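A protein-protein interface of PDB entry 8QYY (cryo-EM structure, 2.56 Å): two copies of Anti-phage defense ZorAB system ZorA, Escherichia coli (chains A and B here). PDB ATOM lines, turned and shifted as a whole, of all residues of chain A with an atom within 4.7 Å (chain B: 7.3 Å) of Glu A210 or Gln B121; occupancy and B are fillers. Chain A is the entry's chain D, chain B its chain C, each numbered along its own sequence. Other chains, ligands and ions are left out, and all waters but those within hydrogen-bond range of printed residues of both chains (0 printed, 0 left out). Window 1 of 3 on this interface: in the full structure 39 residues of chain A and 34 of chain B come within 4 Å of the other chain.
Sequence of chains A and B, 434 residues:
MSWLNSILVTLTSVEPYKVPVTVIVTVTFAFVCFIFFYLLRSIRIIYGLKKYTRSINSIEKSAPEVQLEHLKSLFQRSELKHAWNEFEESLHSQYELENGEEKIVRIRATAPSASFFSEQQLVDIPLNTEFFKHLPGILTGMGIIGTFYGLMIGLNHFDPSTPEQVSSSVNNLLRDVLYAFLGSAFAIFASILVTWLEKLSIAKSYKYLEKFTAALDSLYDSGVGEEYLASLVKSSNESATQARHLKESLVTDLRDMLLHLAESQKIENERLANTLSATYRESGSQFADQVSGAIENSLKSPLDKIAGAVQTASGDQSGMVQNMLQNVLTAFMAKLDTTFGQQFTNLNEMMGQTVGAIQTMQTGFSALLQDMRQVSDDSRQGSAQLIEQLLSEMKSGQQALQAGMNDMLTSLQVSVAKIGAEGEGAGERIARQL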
ATOM      1  N   TYR A 206     -28.097 -12.087 -11.499  1.00  0.00           N
ATOM      2  CA  TYR A 206     -28.349 -10.665 -11.297  1.00  0.00           C
ATOM      3  C   TYR A 206     -28.537  -9.946 -12.627  1.00  0.00           C
ATOM      4  O   TYR A 206     -29.417  -9.087 -12.756  1.00  0.00           O
ATOM      5  CB  TYR A 206     -27.208 -10.044 -10.500  1.00  0.00           C
ATOM      6  CG  TYR A 206     -27.230 -10.439  -9.046  1.00  0.00           C
ATOM      7  CD1 TYR A 206     -28.397 -10.899  -8.454  1.00  0.00           C
ATOM      8  CD2 TYR A 206     -26.085 -10.370  -8.272  1.00  0.00           C
ATOM      9  CE1 TYR A 206     -28.425 -11.267  -7.131  1.00  0.00           C
ATOM     10  CE2 TYR A 206     -26.105 -10.738  -6.946  1.00  0.00           C
ATOM     11  CZ  TYR A 206     -27.278 -11.184  -6.381  1.00  0.00           C
ATOM     12  OH  TYR A 206     -27.300 -11.552  -5.057  1.00  0.00           O
ATOM     13  N   LYS A 207     -27.733 -10.300 -13.632  1.00  0.00           N
ATOM     14  CA  LYS A 207     -27.862  -9.678 -14.947  1.00  0.00           C
ATOM     15  C   LYS A 207     -29.238  -9.931 -15.554  1.00  0.00           C
ATOM     16  O   LYS A 207     -29.887  -9.010 -16.065  1.00  0.00           O
ATOM     17  CB  LYS A 207     -26.765 -10.203 -15.871  1.00  0.00           C
ATOM     18  CG  LYS A 207     -26.845  -9.686 -17.288  1.00  0.00           C
ATOM     19  CD  LYS A 207     -25.954 -10.493 -18.208  1.00  0.00           C
ATOM     20  CE  LYS A 207     -26.101 -10.049 -19.652  1.00  0.00           C
ATOM     21  NZ  LYS A 207     -25.343 -10.935 -20.578  1.00  0.00           N
ATOM     22  N   TYR A 208     -29.701 -11.179 -15.508  1.00  0.00           N
ATOM     23  CA  TYR A 208     -30.974 -11.503 -16.138  1.00  0.00           C
ATOM     24  C   TYR A 208     -32.161 -11.025 -15.316  1.00  0.00           C
ATOM     25  O   TYR A 208     -33.205 -10.686 -15.881  1.00  0.00           O
ATOM     26  CB  TYR A 208     -31.044 -13.001 -16.415  1.00  0.00           C
ATOM     27  CG  TYR A 208     -30.186 -13.381 -17.594  1.00  0.00           C
ATOM     28  CD1 TYR A 208     -30.500 -12.937 -18.868  1.00  0.00           C
ATOM     29  CD2 TYR A 208     -29.032 -14.127 -17.431  1.00  0.00           C
ATOM     30  CE1 TYR A 208     -29.717 -13.260 -19.948  1.00  0.00           C
ATOM     31  CE2 TYR A 208     -28.236 -14.452 -18.508  1.00  0.00           C
ATOM     32  CZ  TYR A 208     -28.585 -14.015 -19.764  1.00  0.00           C
ATOM     33  OH  TYR A 208     -27.798 -14.336 -20.844  1.00  0.00           O
ATOM     34  N   LEU A 209     -32.017 -10.950 -13.993  1.00  0.00           N
ATOM     35  CA  LEU A 209     -33.035 -10.299 -13.181  1.00  0.00           C
ATOM     36  C   LEU A 209     -33.149  -8.823 -13.533  1.00  0.00           C
ATOM     37  O   LEU A 209     -34.254  -8.269 -13.580  1.00  0.00           O
ATOM     38  CB  LEU A 209     -32.707 -10.480 -11.702  1.00  0.00           C
ATOM     39  CG  LEU A 209     -33.657  -9.821 -10.708  1.00  0.00           C
ATOM     40  CD1 LEU A 209     -35.082 -10.216 -11.000  1.00  0.00           C
ATOM     41  CD2 LEU A 209     -33.279 -10.217  -9.310  1.00  0.00           C
ATOM     42  N   GLU A 210     -32.012  -8.161 -13.767  1.00  0.00           N
ATOM     43  CA  GLU A 210     -32.061  -6.772 -14.212  1.00  0.00           C
ATOM     44  C   GLU A 210     -32.717  -6.632 -15.576  1.00  0.00           C
ATOM     45  O   GLU A 210     -33.514  -5.714 -15.789  1.00  0.00           O
ATOM     46  CB  GLU A 210     -30.667  -6.158 -14.230  1.00  0.00           C
ATOM     47  CG  GLU A 210     -30.714  -4.716 -14.665  1.00  0.00           C
ATOM     48  CD  GLU A 210     -31.470  -3.831 -13.705  1.00  0.00           C
ATOM     49  OE1 GLU A 210     -31.542  -4.165 -12.504  1.00  0.00           O
ATOM     50  OE2 GLU A 210     -32.046  -2.826 -14.174  1.00  0.00           O
ATOM     51  N   LYS A 211     -32.391  -7.516 -16.516  1.00  0.00           N
ATOM     52  CA  LYS A 211     -33.057  -7.452 -17.814  1.00  0.00           C
ATOM     53  C   LYS A 211     -34.564  -7.641 -17.665  1.00  0.00           C
ATOM     54  O   LYS A 211     -35.350  -6.934 -18.304  1.00  0.00           O
ATOM     55  CB  LYS A 211     -32.460  -8.485 -18.771  1.00  0.00           C
ATOM     56  CG  LYS A 211     -31.047  -8.152 -19.209  1.00  0.00           C
ATOM     57  CD  LYS A 211     -30.432  -9.264 -20.037  1.00  0.00           C
ATOM     58  CE  LYS A 211     -31.081  -9.361 -21.402  1.00  0.00           C
ATOM     59  NZ  LYS A 211     -30.404 -10.372 -22.260  1.00  0.00           N
ATOM     60  N   PHE A 212     -34.982  -8.559 -16.788  1.00  0.00           N
ATOM     61  CA  PHE A 212     -36.406  -8.800 -16.553  1.00  0.00           C
ATOM     62  C   PHE A 212     -37.101  -7.566 -15.985  1.00  0.00           C
ATOM     63  O   PHE A 212     -38.118  -7.105 -16.520  1.00  0.00           O
ATOM     64  CB  PHE A 212     -36.556  -9.997 -15.612  1.00  0.00           C
ATOM     65  CG  PHE A 212     -37.930 -10.166 -15.024  1.00  0.00           C
ATOM     66  CD1 PHE A 212     -38.951 -10.731 -15.761  1.00  0.00           C
ATOM     67  CD2 PHE A 212     -38.184  -9.807 -13.713  1.00  0.00           C
ATOM     68  CE1 PHE A 212     -40.202 -10.904 -15.214  1.00  0.00           C
ATOM     69  CE2 PHE A 212     -39.433  -9.977 -13.165  1.00  0.00           C
ATOM     70  CZ  PHE A 212     -40.441 -10.528 -13.914  1.00  0.00           C
ATOM     71  N   THR A 213     -36.561  -7.009 -14.901  1.00  0.00           N
ATOM     72  CA  THR A 213     -37.203  -5.856 -14.280  1.00  0.00           C
ATOM     73  C   THR A 213     -37.085  -4.600 -15.127  1.00  0.00           C
ATOM     74  O   THR A 213     -37.877  -3.672 -14.944  1.00  0.00           O
ATOM     75  CB  THR A 213     -36.629  -5.597 -12.889  1.00  0.00           C
ATOM     76  OG1 THR A 213     -35.225  -5.332 -12.987  1.00  0.00           O
ATOM     77  CG2 THR A 213     -36.856  -6.796 -11.996  1.00  0.00           C
ATOM     78  N   ALA A 214     -36.116  -4.538 -16.041  1.00  0.00           N
ATOM     79  CA  ALA A 214     -36.055  -3.425 -16.976  1.00  0.00           C
ATOM     80  C   ALA A 214     -37.088  -3.578 -18.081  1.00  0.00           C
ATOM     81  O   ALA A 214     -37.650  -2.584 -18.550  1.00  0.00           O
ATOM     82  CB  ALA A 214     -34.651  -3.308 -17.564  1.00  0.00           C
ATOM     83  N   GLU B  79     -28.202  -0.276 -22.017  1.00  0.00           N
ATOM     84  CA  GLU B  79     -28.362   0.153 -20.634  1.00  0.00           C
ATOM     85  C   GLU B  79     -28.508   1.668 -20.527  1.00  0.00           C
ATOM     86  O   GLU B  79     -29.363   2.150 -19.777  1.00  0.00           O
ATOM     87  CB  GLU B  79     -27.189  -0.357 -19.793  1.00  0.00           C
ATOM     88  CG  GLU B  79     -25.840   0.226 -20.165  1.00  0.00           C
ATOM     89  CD  GLU B  79     -24.713  -0.357 -19.351  1.00  0.00           C
ATOM     90  OE1 GLU B  79     -24.986  -1.237 -18.512  1.00  0.00           O
ATOM     91  OE2 GLU B  79     -23.553   0.063 -19.550  1.00  0.00           O
ATOM     92  N   LEU B  80     -27.715   2.428 -21.287  1.00  0.00           N
ATOM     93  CA  LEU B  80     -27.864   3.880 -21.294  1.00  0.00           C
ATOM     94  C   LEU B  80     -29.198   4.300 -21.889  1.00  0.00           C
ATOM     95  O   LEU B  80     -29.815   5.254 -21.412  1.00  0.00           O
ATOM     96  CB  LEU B  80     -26.714   4.542 -22.055  1.00  0.00           C
ATOM     97  CG  LEU B  80     -25.384   4.807 -21.345  1.00  0.00           C
ATOM     98  CD1 LEU B  80     -25.572   5.796 -20.211  1.00  0.00           C
ATOM     99  CD2 LEU B  80     -24.750   3.539 -20.834  1.00  0.00           C
ATOM    100  N   HIS B  82     -32.068   2.587 -21.869  1.00  0.00           N
ATOM    101  CA  HIS B  82     -33.097   2.318 -20.870  1.00  0.00           C
ATOM    102  C   HIS B  82     -33.033   3.324 -19.730  1.00  0.00           C
ATOM    103  O   HIS B  82     -34.068   3.840 -19.285  1.00  0.00           O
ATOM    104  CB  HIS B  82     -32.953   0.895 -20.338  1.00  0.00           C
ATOM    105  CG  HIS B  82     -33.891   0.569 -19.216  1.00  0.00           C
ATOM    106  ND1 HIS B  82     -35.223   0.280 -19.419  1.00  0.00           N
ATOM    107  CD2 HIS B  82     -33.688   0.485 -17.881  1.00  0.00           C
ATOM    108  CE1 HIS B  82     -35.799   0.033 -18.257  1.00  0.00           C
ATOM    109  NE2 HIS B  82     -34.890   0.152 -17.307  1.00  0.00           N
ATOM    110  N   ALA B  83     -31.824   3.622 -19.248  1.00  0.00           N
ATOM    111  CA  ALA B  83     -31.676   4.582 -18.163  1.00  0.00           C
ATOM    112  C   ALA B  83     -32.186   5.954 -18.571  1.00  0.00           C
ATOM    113  O   ALA B  83     -32.864   6.626 -17.789  1.00  0.00           O
ATOM    114  CB  ALA B  83     -30.214   4.658 -17.726  1.00  0.00           C
ATOM    115  N   ALA B 114     -29.117   9.787 -10.581  1.00  0.00           N
ATOM    116  CA  ALA B 114     -28.472   8.545 -10.177  1.00  0.00           C
ATOM    117  C   ALA B 114     -29.466   7.430  -9.890  1.00  0.00           C
ATOM    118  O   ALA B 114     -29.050   6.277  -9.754  1.00  0.00           O
ATOM    119  CB  ALA B 114     -27.602   8.786  -8.945  1.00  0.00           C
ATOM    120  N   SER B 115     -30.757   7.743  -9.783  1.00  0.00           N
ATOM    121  CA  SER B 115     -31.757   6.704  -9.579  1.00  0.00           C
ATOM    122  C   SER B 115     -31.873   5.792 -10.790  1.00  0.00           C
ATOM    123  O   SER B 115     -32.296   4.640 -10.662  1.00  0.00           O
ATOM    124  CB  SER B 115     -33.110   7.335  -9.267  1.00  0.00           C
ATOM    125  OG  SER B 115     -33.103   7.951  -7.995  1.00  0.00           O
ATOM    126  N   PHE B 116     -31.507   6.286 -11.963  1.00  0.00           N
ATOM    127  CA  PHE B 116     -31.614   5.539 -13.206  1.00  0.00           C
ATOM    128  C   PHE B 116     -30.266   5.258 -13.845  1.00  0.00           C
ATOM    129  O   PHE B 116     -30.059   4.167 -14.379  1.00  0.00           O
ATOM    130  CB  PHE B 116     -32.514   6.303 -14.182  1.00  0.00           C
ATOM    131  CG  PHE B 116     -33.771   6.826 -13.549  1.00  0.00           C
ATOM    132  CD1 PHE B 116     -34.850   5.990 -13.338  1.00  0.00           C
ATOM    133  CD2 PHE B 116     -33.867   8.148 -13.153  1.00  0.00           C
ATOM    134  CE1 PHE B 116     -36.000   6.459 -12.754  1.00  0.00           C
ATOM    135  CE2 PHE B 116     -35.019   8.622 -12.567  1.00  0.00           C
ATOM    136  CZ  PHE B 116     -36.086   7.777 -12.367  1.00  0.00           C
ATOM    137  N   PHE B 117     -29.345   6.215 -13.803  1.00  0.00           N
ATOM    138  CA  PHE B 117     -27.961   5.989 -14.213  1.00  0.00           C
ATOM    139  C   PHE B 117     -27.123   5.576 -13.004  1.00  0.00           C
ATOM    140  O   PHE B 117     -26.132   6.205 -12.647  1.00  0.00           O
ATOM    141  CB  PHE B 117     -27.396   7.237 -14.874  1.00  0.00           C
ATOM    142  CG  PHE B 117     -28.159   7.686 -16.082  1.00  0.00           C
ATOM    143  CD1 PHE B 117     -29.286   8.477 -15.952  1.00  0.00           C
ATOM    144  CD2 PHE B 117     -27.746   7.323 -17.350  1.00  0.00           C
ATOM    145  CE1 PHE B 117     -29.983   8.893 -17.058  1.00  0.00           C
ATOM    146  CE2 PHE B 117     -28.440   7.740 -18.461  1.00  0.00           C
ATOM    147  CZ  PHE B 117     -29.558   8.527 -18.315  1.00  0.00           C
ATOM    148  N   SER B 118     -27.556   4.499 -12.363  1.00  0.00           N
ATOM    149  CA  SER B 118     -26.948   4.077 -11.114  1.00  0.00           C
ATOM    150  C   SER B 118     -25.711   3.222 -11.368  1.00  0.00           C
ATOM    151  O   SER B 118     -25.477   2.724 -12.469  1.00  0.00           O
ATOM    152  CB  SER B 118     -27.951   3.312 -10.257  1.00  0.00           C
ATOM    153  OG  SER B 118     -28.321   2.103 -10.879  1.00  0.00           O
ATOM    154  N   GLU B 119     -24.916   3.054 -10.310  1.00  0.00           N
ATOM    155  CA  GLU B 119     -23.702   2.252 -10.404  1.00  0.00           C
ATOM    156  C   GLU B 119     -24.019   0.805 -10.745  1.00  0.00           C
ATOM    157  O   GLU B 119     -23.336   0.189 -11.571  1.00  0.00           O
ATOM    158  CB  GLU B 119     -22.928   2.329  -9.096  1.00  0.00           C
ATOM    159  CG  GLU B 119     -22.073   3.557  -8.977  1.00  0.00           C
ATOM    160  CD  GLU B 119     -21.942   4.028  -7.552  1.00  0.00           C
ATOM    161  OE1 GLU B 119     -22.328   3.270  -6.638  1.00  0.00           O
ATOM    162  OE2 GLU B 119     -21.438   5.148  -7.342  1.00  0.00           O
ATOM    163  N   GLN B 120     -25.058   0.250 -10.118  1.00  0.00           N
ATOM    164  CA  GLN B 120     -25.492  -1.108 -10.427  1.00  0.00           C
ATOM    165  C   GLN B 120     -25.870  -1.246 -11.894  1.00  0.00           C
ATOM    166  O   GLN B 120     -25.485  -2.214 -12.559  1.00  0.00           O
ATOM    167  CB  GLN B 120     -26.673  -1.479  -9.534  1.00  0.00           C
ATOM    168  CG  GLN B 120     -27.180  -2.903  -9.684  1.00  0.00           C
ATOM    169  CD  GLN B 120     -28.317  -3.195  -8.722  1.00  0.00           C
ATOM    170  OE1 GLN B 120     -28.825  -4.313  -8.681  1.00  0.00           O
ATOM    171  NE2 GLN B 120     -28.709  -2.201  -7.936  1.00  0.00           N
ATOM    172  N   GLN B 121     -26.625  -0.281 -12.418  1.00  0.00           N
ATOM    173  CA  GLN B 121     -27.149  -0.407 -13.772  1.00  0.00           C
ATOM    174  C   GLN B 121     -26.039  -0.264 -14.804  1.00  0.00           C
ATOM    175  O   GLN B 121     -25.995  -1.002 -15.795  1.00  0.00           O
ATOM    176  CB  GLN B 121     -28.214   0.661 -14.021  1.00  0.00           C
ATOM    177  CG  GLN B 121     -29.443   0.530 -13.155  1.00  0.00           C
ATOM    178  CD  GLN B 121     -30.187  -0.763 -13.370  1.00  0.00           C
ATOM    179  OE1 GLN B 121     -30.178  -1.633 -12.497  1.00  0.00           O
ATOM    180  NE2 GLN B 121     -30.820  -0.910 -14.531  1.00  0.00           N
ATOM    181  N   LEU B 122     -25.128   0.684 -14.584  1.00  0.00           N
ATOM    182  CA  LEU B 122     -24.233   1.155 -15.629  1.00  0.00           C
ATOM    183  C   LEU B 122     -22.798   0.664 -15.493  1.00  0.00           C
ATOM    184  O   LEU B 122     -22.047   0.742 -16.470  1.00  0.00           O
ATOM    185  CB  LEU B 122     -24.219   2.688 -15.660  1.00  0.00           C
ATOM    186  CG  LEU B 122     -25.047   3.398 -16.729  1.00  0.00           C
ATOM    187  CD1 LEU B 122     -26.515   3.174 -16.483  1.00  0.00           C
ATOM    188  CD2 LEU B 122     -24.727   4.877 -16.747  1.00  0.00           C
ATOM    189  N   VAL B 123     -22.385   0.184 -14.321  1.00  0.00           N
ATOM    190  CA  VAL B 123     -21.002  -0.240 -14.136  1.00  0.00           C
ATOM    191  C   VAL B 123     -20.967  -1.672 -13.616  1.00  0.00           C
ATOM    192  O   VAL B 123     -20.285  -2.534 -14.178  1.00  0.00           O
ATOM    193  CB  VAL B 123     -20.263   0.719 -13.184  1.00  0.00           C
ATOM    194  CG1 VAL B 123     -18.924   0.147 -12.791  1.00  0.00           C
ATOM    195  CG2 VAL B 123     -20.097   2.087 -13.824  1.00  0.00           C
ATOM    196  N   ASP B 124     -21.718  -1.934 -12.547  1.00  0.00           N
ATOM    197  CA  ASP B 124     -21.585  -3.199 -11.835  1.00  0.00           C
ATOM    198  C   ASP B 124     -22.042  -4.381 -12.677  1.00  0.00           C
ATOM    199  O   ASP B 124     -21.375  -5.419 -12.704  1.00  0.00           O
ATOM    200  CB  ASP B 124     -22.363  -3.144 -10.523  1.00  0.00           C
ATOM    201  CG  ASP B 124     -21.621  -2.390  -9.443  1.00  0.00           C
ATOM    202  OD1 ASP B 124     -20.456  -2.013  -9.682  1.00  0.00           O
ATOM    203  OD2 ASP B 124     -22.193  -2.168  -8.355  1.00  0.00           O
ATOM    204  N   ILE B 125     -23.171  -4.253 -13.367  1.00  0.00           N
ATOM    205  CA  ILE B 125     -23.718  -5.364 -14.145  1.00  0.00           C
ATOM    206  C   ILE B 125     -22.945  -5.535 -15.450  1.00  0.00           C
ATOM    207  O   ILE B 125     -22.590  -6.673 -15.792  1.00  0.00           O
ATOM    208  CB  ILE B 125     -25.227  -5.186 -14.397  1.00  0.00           C
ATOM    209  CG1 ILE B 125     -26.007  -5.326 -13.091  1.00  0.00           C
ATOM    210  CG2 ILE B 125     -25.726  -6.201 -15.406  1.00  0.00           C
ATOM    211  CD1 ILE B 125     -25.930  -6.699 -12.487  1.00  0.00           C
ATOM    212  N   PRO B 126     -22.666  -4.477 -16.223  1.00  0.00           N
ATOM    213  CA  PRO B 126     -21.829  -4.675 -17.420  1.00  0.00           C
ATOM    214  C   PRO B 126     -20.442  -5.211 -17.122  1.00  0.00           C
ATOM    215  O   PRO B 126     -19.900  -5.970 -17.933  1.00  0.00           O
ATOM    216  CB  PRO B 126     -21.768  -3.274 -18.048  1.00  0.00           C
ATOM    217  CG  PRO B 126     -22.298  -2.355 -17.028  1.00  0.00           C
ATOM    218  CD  PRO B 126     -23.265  -3.133 -16.227  1.00  0.00           C
ATOM    219  N   LEU B 127     -19.842  -4.842 -15.993  1.00  0.00           N
ATOM    220  CA  LEU B 127     -18.499  -5.294 -15.662  1.00  0.00           C
ATOM    221  C   LEU B 127     -18.473  -6.650 -14.975  1.00  0.00           C
ATOM    222  O   LEU B 127     -17.385  -7.199 -14.775  1.00  0.00           O
ATOM    223  CB  LEU B 127     -17.793  -4.270 -14.771  1.00  0.00           C
ATOM    224  CG  LEU B 127     -17.271  -2.999 -15.436  1.00  0.00           C
ATOM    225  CD1 LEU B 127     -16.386  -2.226 -14.478  1.00  0.00           C
ATOM    226  CD2 LEU B 127     -16.528  -3.322 -16.713  1.00  0.00           C
ATOM    227  N   LEU B 209     -18.939   8.307 -13.266  1.00  0.00           N
ATOM    228  CA  LEU B 209     -20.390   8.203 -13.244  1.00  0.00           C
ATOM    229  C   LEU B 209     -20.997   9.276 -12.353  1.00  0.00           C
ATOM    230  O   LEU B 209     -22.057   9.828 -12.671  1.00  0.00           O
ATOM    231  CB  LEU B 209     -20.810   6.810 -12.780  1.00  0.00           C
ATOM    232  CG  LEU B 209     -22.312   6.541 -12.715  1.00  0.00           C
ATOM    233  CD1 LEU B 209     -22.955   6.807 -14.063  1.00  0.00           C
ATOM    234  CD2 LEU B 209     -22.560   5.121 -12.273  1.00  0.00           C
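Among the printed residues, merely in contact across the chains: Ala A214 with His B82 (3.2 Å).
The side-chain amide oxygen (OE1) of Gln B121 sits close to the side-chain carboxylate (OE2) of Glu A210.
Hydrophobic or aromatic side chains of chain A within 4 Å of the printed part of chain B: Ala A214. Printed residues of chain B that touch a printed residue of chain A: His B82 and Gln B121. Among the printed residues, 2 pairs touch across the chains.
Glu A210 touches one residue of chain B. Of the printed residues of chain B, Ala A214 touches His B82. Of the printed residues of chain A, His B82 touches Ala A214. The nearest printed residue of chain A that does not touch His B82 is Glu A210 (5.2 Å).
The backbone carbonyl oxygen of Glu A210 lies within hydrogen-bond range of the side-chain hydroxyl of Thr A213, 3.3 Å away. OG of Ser B118 lies close to N of Gln B121, 3.3 Å away.
1 position is printed for both chains. Of the 2 pairs that touch across the chains among the printed residues, none has its exchanged pair printed and touching as well.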
